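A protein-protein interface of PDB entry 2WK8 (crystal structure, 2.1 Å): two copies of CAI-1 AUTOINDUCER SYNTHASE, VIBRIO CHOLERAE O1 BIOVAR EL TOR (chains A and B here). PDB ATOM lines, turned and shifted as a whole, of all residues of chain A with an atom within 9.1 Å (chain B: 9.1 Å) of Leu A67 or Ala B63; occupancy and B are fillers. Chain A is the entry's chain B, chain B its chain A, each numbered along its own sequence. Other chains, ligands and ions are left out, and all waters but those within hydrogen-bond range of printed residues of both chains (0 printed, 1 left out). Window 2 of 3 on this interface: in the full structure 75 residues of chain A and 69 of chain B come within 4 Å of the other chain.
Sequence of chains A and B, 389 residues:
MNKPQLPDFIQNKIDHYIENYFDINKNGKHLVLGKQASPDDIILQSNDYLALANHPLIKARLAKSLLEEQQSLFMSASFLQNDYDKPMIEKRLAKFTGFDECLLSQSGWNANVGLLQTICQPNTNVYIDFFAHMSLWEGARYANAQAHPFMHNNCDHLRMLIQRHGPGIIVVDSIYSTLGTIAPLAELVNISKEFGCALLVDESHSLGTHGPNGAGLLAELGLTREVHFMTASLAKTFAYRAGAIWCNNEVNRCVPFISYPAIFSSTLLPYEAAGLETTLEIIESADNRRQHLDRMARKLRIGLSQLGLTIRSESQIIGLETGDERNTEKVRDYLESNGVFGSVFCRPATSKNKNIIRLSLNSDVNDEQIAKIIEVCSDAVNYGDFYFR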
ATOM      1  N   LYS A  59      12.135   5.536 -12.491  1.00  0.00           N
ATOM      2  CA  LYS A  59      11.838   6.845 -11.933  1.00  0.00           C
ATOM      3  C   LYS A  59      11.568   6.715 -10.426  1.00  0.00           C
ATOM      4  O   LYS A  59      12.161   7.413  -9.612  1.00  0.00           O
ATOM      5  CB  LYS A  59      10.671   7.494 -12.690  1.00  0.00           C
ATOM      6  CG  LYS A  59      10.983   7.709 -14.169  1.00  0.00           C
ATOM      7  CD  LYS A  59      10.152   8.800 -14.794  1.00  0.00           C
ATOM      8  CE  LYS A  59       8.669   8.555 -14.576  1.00  0.00           C
ATOM      9  NZ  LYS A  59       7.837   9.488 -15.373  1.00  0.00           N
ATOM     10  N   ALA A  60      10.703   5.773 -10.064  1.00  0.00           N
ATOM     11  CA  ALA A  60      10.415   5.492  -8.661  1.00  0.00           C
ATOM     12  C   ALA A  60      11.672   5.255  -7.834  1.00  0.00           C
ATOM     13  O   ALA A  60      11.869   5.900  -6.811  1.00  0.00           O
ATOM     14  CB  ALA A  60       9.465   4.301  -8.535  1.00  0.00           C
ATOM     15  N   ARG A  61      12.514   4.317  -8.259  1.00  0.00           N
ATOM     16  CA  ARG A  61      13.739   4.034  -7.526  1.00  0.00           C
ATOM     17  C   ARG A  61      14.641   5.271  -7.353  1.00  0.00           C
ATOM     18  O   ARG A  61      15.234   5.474  -6.294  1.00  0.00           O
ATOM     19  CB  ARG A  61      14.514   2.904  -8.201  1.00  0.00           C
ATOM     20  CG  ARG A  61      15.812   2.506  -7.475  1.00  0.00           C
ATOM     21  CD  ARG A  61      15.543   1.600  -6.280  1.00  0.00           C
ATOM     22  NE  ARG A  61      16.788   1.181  -5.629  1.00  0.00           N
ATOM     23  CZ  ARG A  61      17.488   0.103  -5.978  1.00  0.00           C
ATOM     24  NH1 ARG A  61      17.071  -0.672  -6.971  1.00  0.00           N
ATOM     25  NH2 ARG A  61      18.607  -0.205  -5.332  1.00  0.00           N
ATOM     26  N   LEU A  62      14.747   6.095  -8.395  1.00  0.00           N
ATOM     27  CA  LEU A  62      15.553   7.320  -8.330  1.00  0.00           C
ATOM     28  C   LEU A  62      15.014   8.334  -7.323  1.00  0.00           C
ATOM     29  O   LEU A  62      15.752   8.828  -6.453  1.00  0.00           O
ATOM     30  CB  LEU A  62      15.628   7.981  -9.708  1.00  0.00           C
ATOM     31  CG  LEU A  62      16.881   7.712 -10.538  1.00  0.00           C
ATOM     32  CD1 LEU A  62      16.823   8.505 -11.830  1.00  0.00           C
ATOM     33  CD2 LEU A  62      18.133   8.064  -9.747  1.00  0.00           C
ATOM     34  N   ALA A  63      13.731   8.662  -7.466  1.00  0.00           N
ATOM     35  CA  ALA A  63      13.082   9.606  -6.561  1.00  0.00           C
ATOM     36  C   ALA A  63      13.197   9.100  -5.127  1.00  0.00           C
ATOM     37  O   ALA A  63      13.620   9.826  -4.226  1.00  0.00           O
ATOM     38  CB  ALA A  63      11.622   9.804  -6.950  1.00  0.00           C
ATOM     39  N   LYS A  64      12.844   7.834  -4.929  1.00  0.00           N
ATOM     40  CA  LYS A  64      12.909   7.227  -3.611  1.00  0.00           C
ATOM     41  C   LYS A  64      14.242   7.551  -2.977  1.00  0.00           C
ATOM     42  O   LYS A  64      14.301   8.064  -1.849  1.00  0.00           O
ATOM     43  CB  LYS A  64      12.751   5.705  -3.697  1.00  0.00           C
ATOM     44  CG  LYS A  64      12.075   5.065  -2.499  1.00  0.00           C
ATOM     45  CD  LYS A  64      12.494   3.592  -2.291  1.00  0.00           C
ATOM     46  CE  LYS A  64      12.531   2.786  -3.593  1.00  0.00           C
ATOM     47  NZ  LYS A  64      11.216   2.248  -4.042  1.00  0.00           N
ATOM     48  N   SER A  65      15.314   7.250  -3.707  1.00  0.00           N
ATOM     49  CA  SER A  65      16.661   7.370  -3.154  1.00  0.00           C
ATOM     50  C   SER A  65      17.119   8.812  -3.059  1.00  0.00           C
ATOM     51  O   SER A  65      17.959   9.146  -2.226  1.00  0.00           O
ATOM     52  CB  SER A  65      17.672   6.528  -3.945  1.00  0.00           C
ATOM     53  OG  SER A  65      17.668   5.189  -3.465  1.00  0.00           O
ATOM     54  N   LEU A  66      16.587   9.667  -3.917  1.00  0.00           N
ATOM     55  CA  LEU A  66      16.971  11.065  -3.827  1.00  0.00           C
ATOM     56  C   LEU A  66      16.224  11.736  -2.677  1.00  0.00           C
ATOM     57  O   LEU A  66      16.767  12.623  -2.026  1.00  0.00           O
ATOM     58  CB  LEU A  66      16.771  11.789  -5.153  1.00  0.00           C
ATOM     59  CG  LEU A  66      15.467  12.533  -5.357  1.00  0.00           C
ATOM     60  CD1 LEU A  66      15.570  13.882  -4.680  1.00  0.00           C
ATOM     61  CD2 LEU A  66      15.234  12.697  -6.844  1.00  0.00           C
ATOM     62  N   LEU A  67      14.989  11.305  -2.421  1.00  0.00           N
ATOM     63  CA  LEU A  67      14.322  11.646  -1.164  1.00  0.00           C
ATOM     64  C   LEU A  67      15.074  10.923  -0.060  1.00  0.00           C
ATOM     65  O   LEU A  67      15.687   9.904  -0.311  1.00  0.00           O
ATOM     66  CB  LEU A  67      12.852  11.220  -1.180  1.00  0.00           C
ATOM     67  CG  LEU A  67      11.863  12.181  -1.827  1.00  0.00           C
ATOM     68  CD1 LEU A  67      12.375  13.612  -1.736  1.00  0.00           C
ATOM     69  CD2 LEU A  67      11.584  11.812  -3.264  1.00  0.00           C
ATOM     70  N   GLU A  68      15.033  11.450   1.155  1.00  0.00           N
ATOM     71  CA  GLU A  68      15.929  10.982   2.212  1.00  0.00           C
ATOM     72  C   GLU A  68      17.383  11.392   1.950  1.00  0.00           C
ATOM     73  O   GLU A  68      18.282  11.047   2.723  1.00  0.00           O
ATOM     74  CB  GLU A  68      15.858   9.465   2.375  1.00  0.00           C
ATOM     75  CG  GLU A  68      16.940   8.698   1.618  1.00  0.00           C
ATOM     76  CD  GLU A  68      16.855   7.207   1.863  1.00  0.00           C
ATOM     77  OE1 GLU A  68      17.012   6.435   0.887  1.00  0.00           O
ATOM     78  OE2 GLU A  68      16.620   6.808   3.031  1.00  0.00           O
ATOM     79  N   TYR A 271      22.886   8.729  -4.649  1.00  0.00           N
ATOM     80  CA  TYR A 271      21.567   8.289  -5.070  1.00  0.00           C
ATOM     81  C   TYR A 271      21.542   8.004  -6.571  1.00  0.00           C
ATOM     82  O   TYR A 271      20.650   7.303  -7.063  1.00  0.00           O
ATOM     83  CB  TYR A 271      20.486   9.301  -4.682  1.00  0.00           C
ATOM     84  CG  TYR A 271      20.532  10.604  -5.440  1.00  0.00           C
ATOM     85  CD1 TYR A 271      20.029  10.701  -6.735  1.00  0.00           C
ATOM     86  CD2 TYR A 271      21.049  11.737  -4.857  1.00  0.00           C
ATOM     87  CE1 TYR A 271      20.059  11.887  -7.422  1.00  0.00           C
ATOM     88  CE2 TYR A 271      21.083  12.939  -5.538  1.00  0.00           C
ATOM     89  CZ  TYR A 271      20.590  13.007  -6.815  1.00  0.00           C
ATOM     90  OH  TYR A 271      20.630  14.207  -7.472  1.00  0.00           O
ATOM     91  N   ALA B  53      22.736  20.366   0.603  1.00  0.00           N
ATOM     92  CA  ALA B  53      22.773  19.012   0.044  1.00  0.00           C
ATOM     93  C   ALA B  53      21.489  18.252   0.297  1.00  0.00           C
ATOM     94  O   ALA B  53      21.033  17.493  -0.554  1.00  0.00           O
ATOM     95  CB  ALA B  53      23.940  18.225   0.627  1.00  0.00           C
ATOM     96  N   ASN B  54      20.934  18.437   1.488  1.00  0.00           N
ATOM     97  CA  ASN B  54      19.773  17.676   1.916  1.00  0.00           C
ATOM     98  C   ASN B  54      18.545  18.535   2.097  1.00  0.00           C
ATOM     99  O   ASN B  54      17.623  18.169   2.825  1.00  0.00           O
ATOM    100  CB  ASN B  54      20.064  16.928   3.211  1.00  0.00           C
ATOM    101  CG  ASN B  54      20.298  15.457   2.976  1.00  0.00           C
ATOM    102  OD1 ASN B  54      19.419  14.628   3.247  1.00  0.00           O
ATOM    103  ND2 ASN B  54      21.476  15.118   2.442  1.00  0.00           N
ATOM    104  N   HIS B  55      18.533  19.681   1.432  1.00  0.00           N
ATOM    105  CA  HIS B  55      17.412  20.587   1.559  1.00  0.00           C
ATOM    106  C   HIS B  55      16.137  19.933   1.026  1.00  0.00           C
ATOM    107  O   HIS B  55      16.097  19.431  -0.098  1.00  0.00           O
ATOM    108  CB  HIS B  55      17.703  21.900   0.858  1.00  0.00           C
ATOM    109  CG  HIS B  55      16.778  23.003   1.257  1.00  0.00           C
ATOM    110  ND1 HIS B  55      15.456  23.034   0.873  1.00  0.00           N
ATOM    111  CD2 HIS B  55      16.981  24.115   2.007  1.00  0.00           C
ATOM    112  CE1 HIS B  55      14.886  24.122   1.358  1.00  0.00           C
ATOM    113  NE2 HIS B  55      15.788  24.795   2.050  1.00  0.00           N
ATOM    114  N   PRO B  56      15.090  19.920   1.849  1.00  0.00           N
ATOM    115  CA  PRO B  56      13.836  19.224   1.541  1.00  0.00           C
ATOM    116  C   PRO B  56      13.105  19.801   0.321  1.00  0.00           C
ATOM    117  O   PRO B  56      12.607  19.057  -0.515  1.00  0.00           O
ATOM    118  CB  PRO B  56      13.011  19.424   2.815  1.00  0.00           C
ATOM    119  CG  PRO B  56      14.025  19.704   3.873  1.00  0.00           C
ATOM    120  CD  PRO B  56      15.085  20.492   3.201  1.00  0.00           C
ATOM    121  N   LEU B  57      13.061  21.121   0.213  1.00  0.00           N
ATOM    122  CA  LEU B  57      12.447  21.750  -0.944  1.00  0.00           C
ATOM    123  C   LEU B  57      13.154  21.367  -2.259  1.00  0.00           C
ATOM    124  O   LEU B  57      12.512  21.176  -3.290  1.00  0.00           O
ATOM    125  CB  LEU B  57      12.416  23.271  -0.759  1.00  0.00           C
ATOM    126  CG  LEU B  57      11.475  24.038  -1.686  1.00  0.00           C
ATOM    127  CD1 LEU B  57      10.057  23.490  -1.585  1.00  0.00           C
ATOM    128  CD2 LEU B  57      11.505  25.523  -1.366  1.00  0.00           C
ATOM    129  N   ILE B  58      14.478  21.253  -2.222  1.00  0.00           N
ATOM    130  CA  ILE B  58      15.231  20.881  -3.412  1.00  0.00           C
ATOM    131  C   ILE B  58      14.934  19.440  -3.786  1.00  0.00           C
ATOM    132  O   ILE B  58      14.569  19.141  -4.923  1.00  0.00           O
ATOM    133  CB  ILE B  58      16.758  21.114  -3.208  1.00  0.00           C
ATOM    134  CG1 ILE B  58      17.060  22.609  -3.316  1.00  0.00           C
ATOM    135  CG2 ILE B  58      17.583  20.345  -4.230  1.00  0.00           C
ATOM    136  CD1 ILE B  58      18.410  23.035  -2.786  1.00  0.00           C
ATOM    137  N   LYS B  59      15.063  18.543  -2.819  1.00  0.00           N
ATOM    138  CA  LYS B  59      14.880  17.130  -3.103  1.00  0.00           C
ATOM    139  C   LYS B  59      13.460  16.875  -3.599  1.00  0.00           C
ATOM    140  O   LYS B  59      13.241  16.096  -4.531  1.00  0.00           O
ATOM    141  CB  LYS B  59      15.235  16.289  -1.877  1.00  0.00           C
ATOM    142  CG  LYS B  59      16.554  16.733  -1.245  1.00  0.00           C
ATOM    143  CD  LYS B  59      17.254  15.620  -0.471  1.00  0.00           C
ATOM    144  CE  LYS B  59      16.506  15.287   0.813  1.00  0.00           C
ATOM    145  NZ  LYS B  59      17.228  14.265   1.626  1.00  0.00           N
ATOM    146  N   ALA B  60      12.507  17.583  -3.004  1.00  0.00           N
ATOM    147  CA  ALA B  60      11.102  17.414  -3.351  1.00  0.00           C
ATOM    148  C   ALA B  60      10.830  17.842  -4.779  1.00  0.00           C
ATOM    149  O   ALA B  60      10.066  17.209  -5.495  1.00  0.00           O
ATOM    150  CB  ALA B  60      10.228  18.193  -2.381  1.00  0.00           C
ATOM    151  N   ARG B  61      11.471  18.924  -5.202  1.00  0.00           N
ATOM    152  CA  ARG B  61      11.266  19.443  -6.545  1.00  0.00           C
ATOM    153  C   ARG B  61      11.975  18.618  -7.612  1.00  0.00           C
ATOM    154  O   ARG B  61      11.505  18.512  -8.753  1.00  0.00           O
ATOM    155  CB  ARG B  61      11.723  20.888  -6.608  1.00  0.00           C
ATOM    156  CG  ARG B  61      11.063  21.768  -5.566  1.00  0.00           C
ATOM    157  CD  ARG B  61       9.566  21.950  -5.804  1.00  0.00           C
ATOM    158  NE  ARG B  61       9.024  22.985  -4.923  1.00  0.00           N
ATOM    159  CZ  ARG B  61       8.895  24.273  -5.248  1.00  0.00           C
ATOM    160  NH1 ARG B  61       9.254  24.704  -6.451  1.00  0.00           N
ATOM    161  NH2 ARG B  61       8.398  25.137  -4.367  1.00  0.00           N
ATOM    162  N   LEU B  62      13.130  18.063  -7.254  1.00  0.00           N
ATOM    163  CA  LEU B  62      13.828  17.145  -8.142  1.00  0.00           C
ATOM    164  C   LEU B  62      12.941  15.942  -8.385  1.00  0.00           C
ATOM    165  O   LEU B  62      12.701  15.550  -9.529  1.00  0.00           O
ATOM    166  CB  LEU B  62      15.131  16.664  -7.503  1.00  0.00           C
ATOM    167  CG  LEU B  62      16.433  17.275  -8.000  1.00  0.00           C
ATOM    168  CD1 LEU B  62      17.590  16.750  -7.193  1.00  0.00           C
ATOM    169  CD2 LEU B  62      16.622  16.955  -9.476  1.00  0.00           C
ATOM    170  N   ALA B  63      12.458  15.356  -7.292  1.00  0.00           N
ATOM    171  CA  ALA B  63      11.592  14.182  -7.376  1.00  0.00           C
ATOM    172  C   ALA B  63      10.358  14.495  -8.219  1.00  0.00           C
ATOM    173  O   ALA B  63       9.969  13.706  -9.081  1.00  0.00           O
ATOM    174  CB  ALA B  63      11.194  13.727  -5.994  1.00  0.00           C
ATOM    175  N   LYS B  64       9.768  15.667  -7.984  1.00  0.00           N
ATOM    176  CA  LYS B  64       8.562  16.074  -8.701  1.00  0.00           C
ATOM    177  C   LYS B  64       8.740  16.081 -10.219  1.00  0.00           C
ATOM    178  O   LYS B  64       7.965  15.453 -10.937  1.00  0.00           O
ATOM    179  CB  LYS B  64       8.077  17.448  -8.238  1.00  0.00           C
ATOM    180  CG  LYS B  64       6.605  17.725  -8.560  1.00  0.00           C
ATOM    181  CD  LYS B  64       6.335  19.205  -8.856  1.00  0.00           C
ATOM    182  CE  LYS B  64       6.517  19.532 -10.347  1.00  0.00           C
ATOM    183  NZ  LYS B  64       5.556  18.820 -11.249  1.00  0.00           N
ATOM    184  N   SER B  65       9.747  16.805 -10.710  1.00  0.00           N
ATOM    185  CA  SER B  65       9.932  16.967 -12.155  1.00  0.00           C
ATOM    186  C   SER B  65      10.325  15.642 -12.785  1.00  0.00           C
ATOM    187  O   SER B  65       9.911  15.319 -13.905  1.00  0.00           O
ATOM    188  CB  SER B  65      10.980  18.051 -12.471  1.00  0.00           C
ATOM    189  OG  SER B  65      12.256  17.701 -11.955  1.00  0.00           O
ATOM    190  N   LEU B  66      11.123  14.889 -12.037  1.00  0.00           N
ATOM    191  CA  LEU B  66      11.574  13.559 -12.396  1.00  0.00           C
ATOM    192  C   LEU B  66      10.404  12.617 -12.732  1.00  0.00           C
ATOM    193  O   LEU B  66      10.604  11.549 -13.316  1.00  0.00           O
ATOM    194  CB  LEU B  66      12.395  13.009 -11.234  1.00  0.00           C
ATOM    195  CG  LEU B  66      13.346  11.838 -11.406  1.00  0.00           C
ATOM    196  CD1 LEU B  66      14.357  11.829 -10.256  1.00  0.00           C
ATOM    197  CD2 LEU B  66      12.559  10.547 -11.447  1.00  0.00           C
ATOM    198  N   LEU B  67       9.184  13.017 -12.370  1.00  0.00           N
ATOM    199  CA  LEU B  67       7.994  12.316 -12.846  1.00  0.00           C
ATOM    200  C   LEU B  67       7.291  13.105 -13.973  1.00  0.00           C
ATOM    201  O   LEU B  67       7.159  14.335 -13.917  1.00  0.00           O
ATOM    202  CB  LEU B  67       7.044  12.010 -11.688  1.00  0.00           C
ATOM    203  CG  LEU B  67       7.734  11.799 -10.330  1.00  0.00           C
ATOM    204  CD1 LEU B  67       6.727  11.532  -9.230  1.00  0.00           C
ATOM    205  CD2 LEU B  67       8.746  10.677 -10.379  1.00  0.00           C
ATOM    206  N   GLU B  68       6.894  12.373 -15.012  1.00  0.00           N
ATOM    207  CA  GLU B  68       6.185  12.913 -16.173  1.00  0.00           C
ATOM    208  C   GLU B  68       7.057  13.262 -17.375  1.00  0.00           C
ATOM    209  O   GLU B  68       6.667  14.087 -18.206  1.00  0.00           O
ATOM    210  CB  GLU B  68       5.288  14.099 -15.802  1.00  0.00           C
ATOM    211  CG  GLU B  68       3.863  13.694 -15.488  1.00  0.00           C
ATOM    212  CD  GLU B  68       2.853  14.498 -16.264  1.00  0.00           C
ATOM    213  OE1 GLU B  68       3.283  15.378 -17.035  1.00  0.00           O
ATOM    214  OE2 GLU B  68       1.635  14.248 -16.117  1.00  0.00           O
ATOM    215  N   GLU B  69       8.220  12.627 -17.486  1.00  0.00           N
ATOM    216  CA  GLU B  69       9.097  12.866 -18.624  1.00  0.00           C
ATOM    217  C   GLU B  69       8.299  12.682 -19.888  1.00  0.00           C
ATOM    218  O   GLU B  69       7.310  11.947 -19.890  1.00  0.00           O
ATOM    219  CB  GLU B  69      10.246  11.842 -18.669  1.00  0.00           C
ATOM    220  CG  GLU B  69      11.021  11.698 -17.385  1.00  0.00           C
ATOM    221  CD  GLU B  69      11.210  13.030 -16.717  1.00  0.00           C
ATOM    222  OE1 GLU B  69      10.748  13.177 -15.562  1.00  0.00           O
ATOM    223  OE2 GLU B  69      11.787  13.935 -17.360  1.00  0.00           O
ATOM    224  N   TYR B 271      14.848  17.285 -16.103  1.00  0.00           N
ATOM    225  CA  TYR B 271      14.500  17.375 -14.687  1.00  0.00           C
ATOM    226  C   TYR B 271      15.637  17.925 -13.829  1.00  0.00           C
ATOM    227  O   TYR B 271      15.395  18.547 -12.796  1.00  0.00           O
ATOM    228  CB  TYR B 271      14.000  16.037 -14.138  1.00  0.00           C
ATOM    229  CG  TYR B 271      15.079  15.011 -13.865  1.00  0.00           C
ATOM    230  CD1 TYR B 271      15.757  14.989 -12.648  1.00  0.00           C
ATOM    231  CD2 TYR B 271      15.394  14.051 -14.808  1.00  0.00           C
ATOM    232  CE1 TYR B 271      16.730  14.046 -12.396  1.00  0.00           C
ATOM    233  CE2 TYR B 271      16.365  13.114 -14.565  1.00  0.00           C
ATOM    234  CZ  TYR B 271      17.026  13.113 -13.361  1.00  0.00           C
ATOM    235  OH  TYR B 271      17.975  12.149 -13.127  1.00  0.00           O
ATOM    236  N   GLU B 272      16.876  17.702 -14.256  1.00  0.00           N
ATOM    237  CA  GLU B 272      18.018  18.248 -13.531  1.00  0.00           C
ATOM    238  C   GLU B 272      17.927  19.773 -13.456  1.00  0.00           C
ATOM    239  O   GLU B 272      18.100  20.353 -12.393  1.00  0.00           O
ATOM    240  CB  GLU B 272      19.342  17.775 -14.140  1.00  0.00           C
ATOM    241  CG  GLU B 272      19.355  16.280 -14.416  1.00  0.00           C
ATOM    242  CD  GLU B 272      20.739  15.741 -14.690  1.00  0.00           C
ATOM    243  OE1 GLU B 272      21.532  15.760 -13.746  1.00  0.00           O
ATOM    244  OE2 GLU B 272      21.029  15.290 -15.826  1.00  0.00           O
ATOM    245  N   ALA B 274      15.311  21.565 -13.517  1.00  0.00           N
ATOM    246  CA  ALA B 274      14.181  21.975 -12.697  1.00  0.00           C
ATOM    247  C   ALA B 274      14.599  22.091 -11.245  1.00  0.00           C
ATOM    248  O   ALA B 274      14.159  22.994 -10.540  1.00  0.00           O
ATOM    249  CB  ALA B 274      13.025  20.990 -12.850  1.00  0.00           C
ATOM    250  N   GLY B 275      15.439  21.160 -10.800  1.00  0.00           N
ATOM    251  CA  GLY B 275      15.992  21.223  -9.462  1.00  0.00           C
ATOM    252  C   GLY B 275      16.830  22.475  -9.275  1.00  0.00           C
ATOM    253  O   GLY B 275      16.717  23.188  -8.274  1.00  0.00           O
ATOM    254  N   THR B 278      14.878  25.565  -8.263  1.00  0.00           N
ATOM    255  CA  THR B 278      14.534  25.635  -6.859  1.00  0.00           C
ATOM    256  C   THR B 278      15.773  25.957  -6.022  1.00  0.00           C
ATOM    257  O   THR B 278      15.705  26.780  -5.104  1.00  0.00           O
ATOM    258  CB  THR B 278      13.832  24.340  -6.389  1.00  0.00           C
ATOM    259  OG1 THR B 278      12.569  24.218  -7.066  1.00  0.00           O
ATOM    260  CG2 THR B 278      13.610  24.368  -4.869  1.00  0.00           C
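The side-chain amino group of Lys B59 is in hydrogen-bond range of the side-chain amide oxygen of Asn B54 (2.7 Å).
OG of Ser B65 sits at hydrogen-bond distance from O of Leu B62, at 3.3 Å.
N of Glu B68 lies close to NZ of Lys A59.
Of the 11 printed residues of chain A, 5 touch a printed residue of chain B.
Hydrophobic or aromatic side chains of chain A within 4 Å of the printed part of chain B: Leu A66, Leu A67 and Tyr A271.
Of the 22 printed residues of chain B, 8 touch a printed residue of chain A.
Hydrophobic or aromatic side chains of chain B that line the printed part of chain A: Leu B62, Ala B63 and Leu B66.
Lys A59 touches Glu B68, and with the chains exchanged Glu A68 touches Lys B59.
Leu A66 touches Leu B62, but with the chains exchanged Leu A62 does not touch Leu B66 (4.1 Å).
Leu A66 touches its own counterpart, Leu B66.
Tyr A271 touches Leu B62, but with the chains exchanged Leu A62 does not touch Tyr B271 (4.04 Å).
Leu A67 touches just these residues of chain B: Lys B59 and Ala B63.
Of chain B, only Asn B54 and Lys B59 come within 4 Å of Glu A68.
Leu B57 touches none of the printed residues of chain A.
Printed residues of chain A within 4 Å of Lys B59: Leu A66, Leu A67 and Glu A68.
Printed residues of chain A within 4 Å of Leu B62: Leu A66 and Tyr A271.
Of chain A, only Leu A66 (3.9 Å) and Leu A67 (3.4 Å) come within 4 Å of Ala B63.
Printed residues of chain A within 4 Å of Glu B69: Lys A59 (3.8 Å).
Ala B274 touches none of the printed residues of chain A.
The nearest printed residue of chain A that does not touch Asn B54 is Leu A66 (6.2 Å).
Lys A59 touches Leu B67 (NZ to CA, 3.8 Å).
Glu B69 touches Lys A59 (N to NZ, 3.8 Å).
Lys B59 touches Leu A66 (O to CD1, 3.2 Å).
Leu A66 touches Leu B62 (CD1 to CB, 3.99 Å).
Leu A66 touches Ala B63.
CD2 of Leu A66 touches CD1 of Leu B66 (3.6 Å).
O of Lys B59 touches CD1 of Leu A67 (3.8 Å).
Ala B63 touches Leu A67 (CB to CD2, 3.4 Å).
Asn B54 touches Glu A68 (OD1 to O, 3.8 Å).
CD1 of Leu B62 touches OH of Tyr A271, at 3.97 Å.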
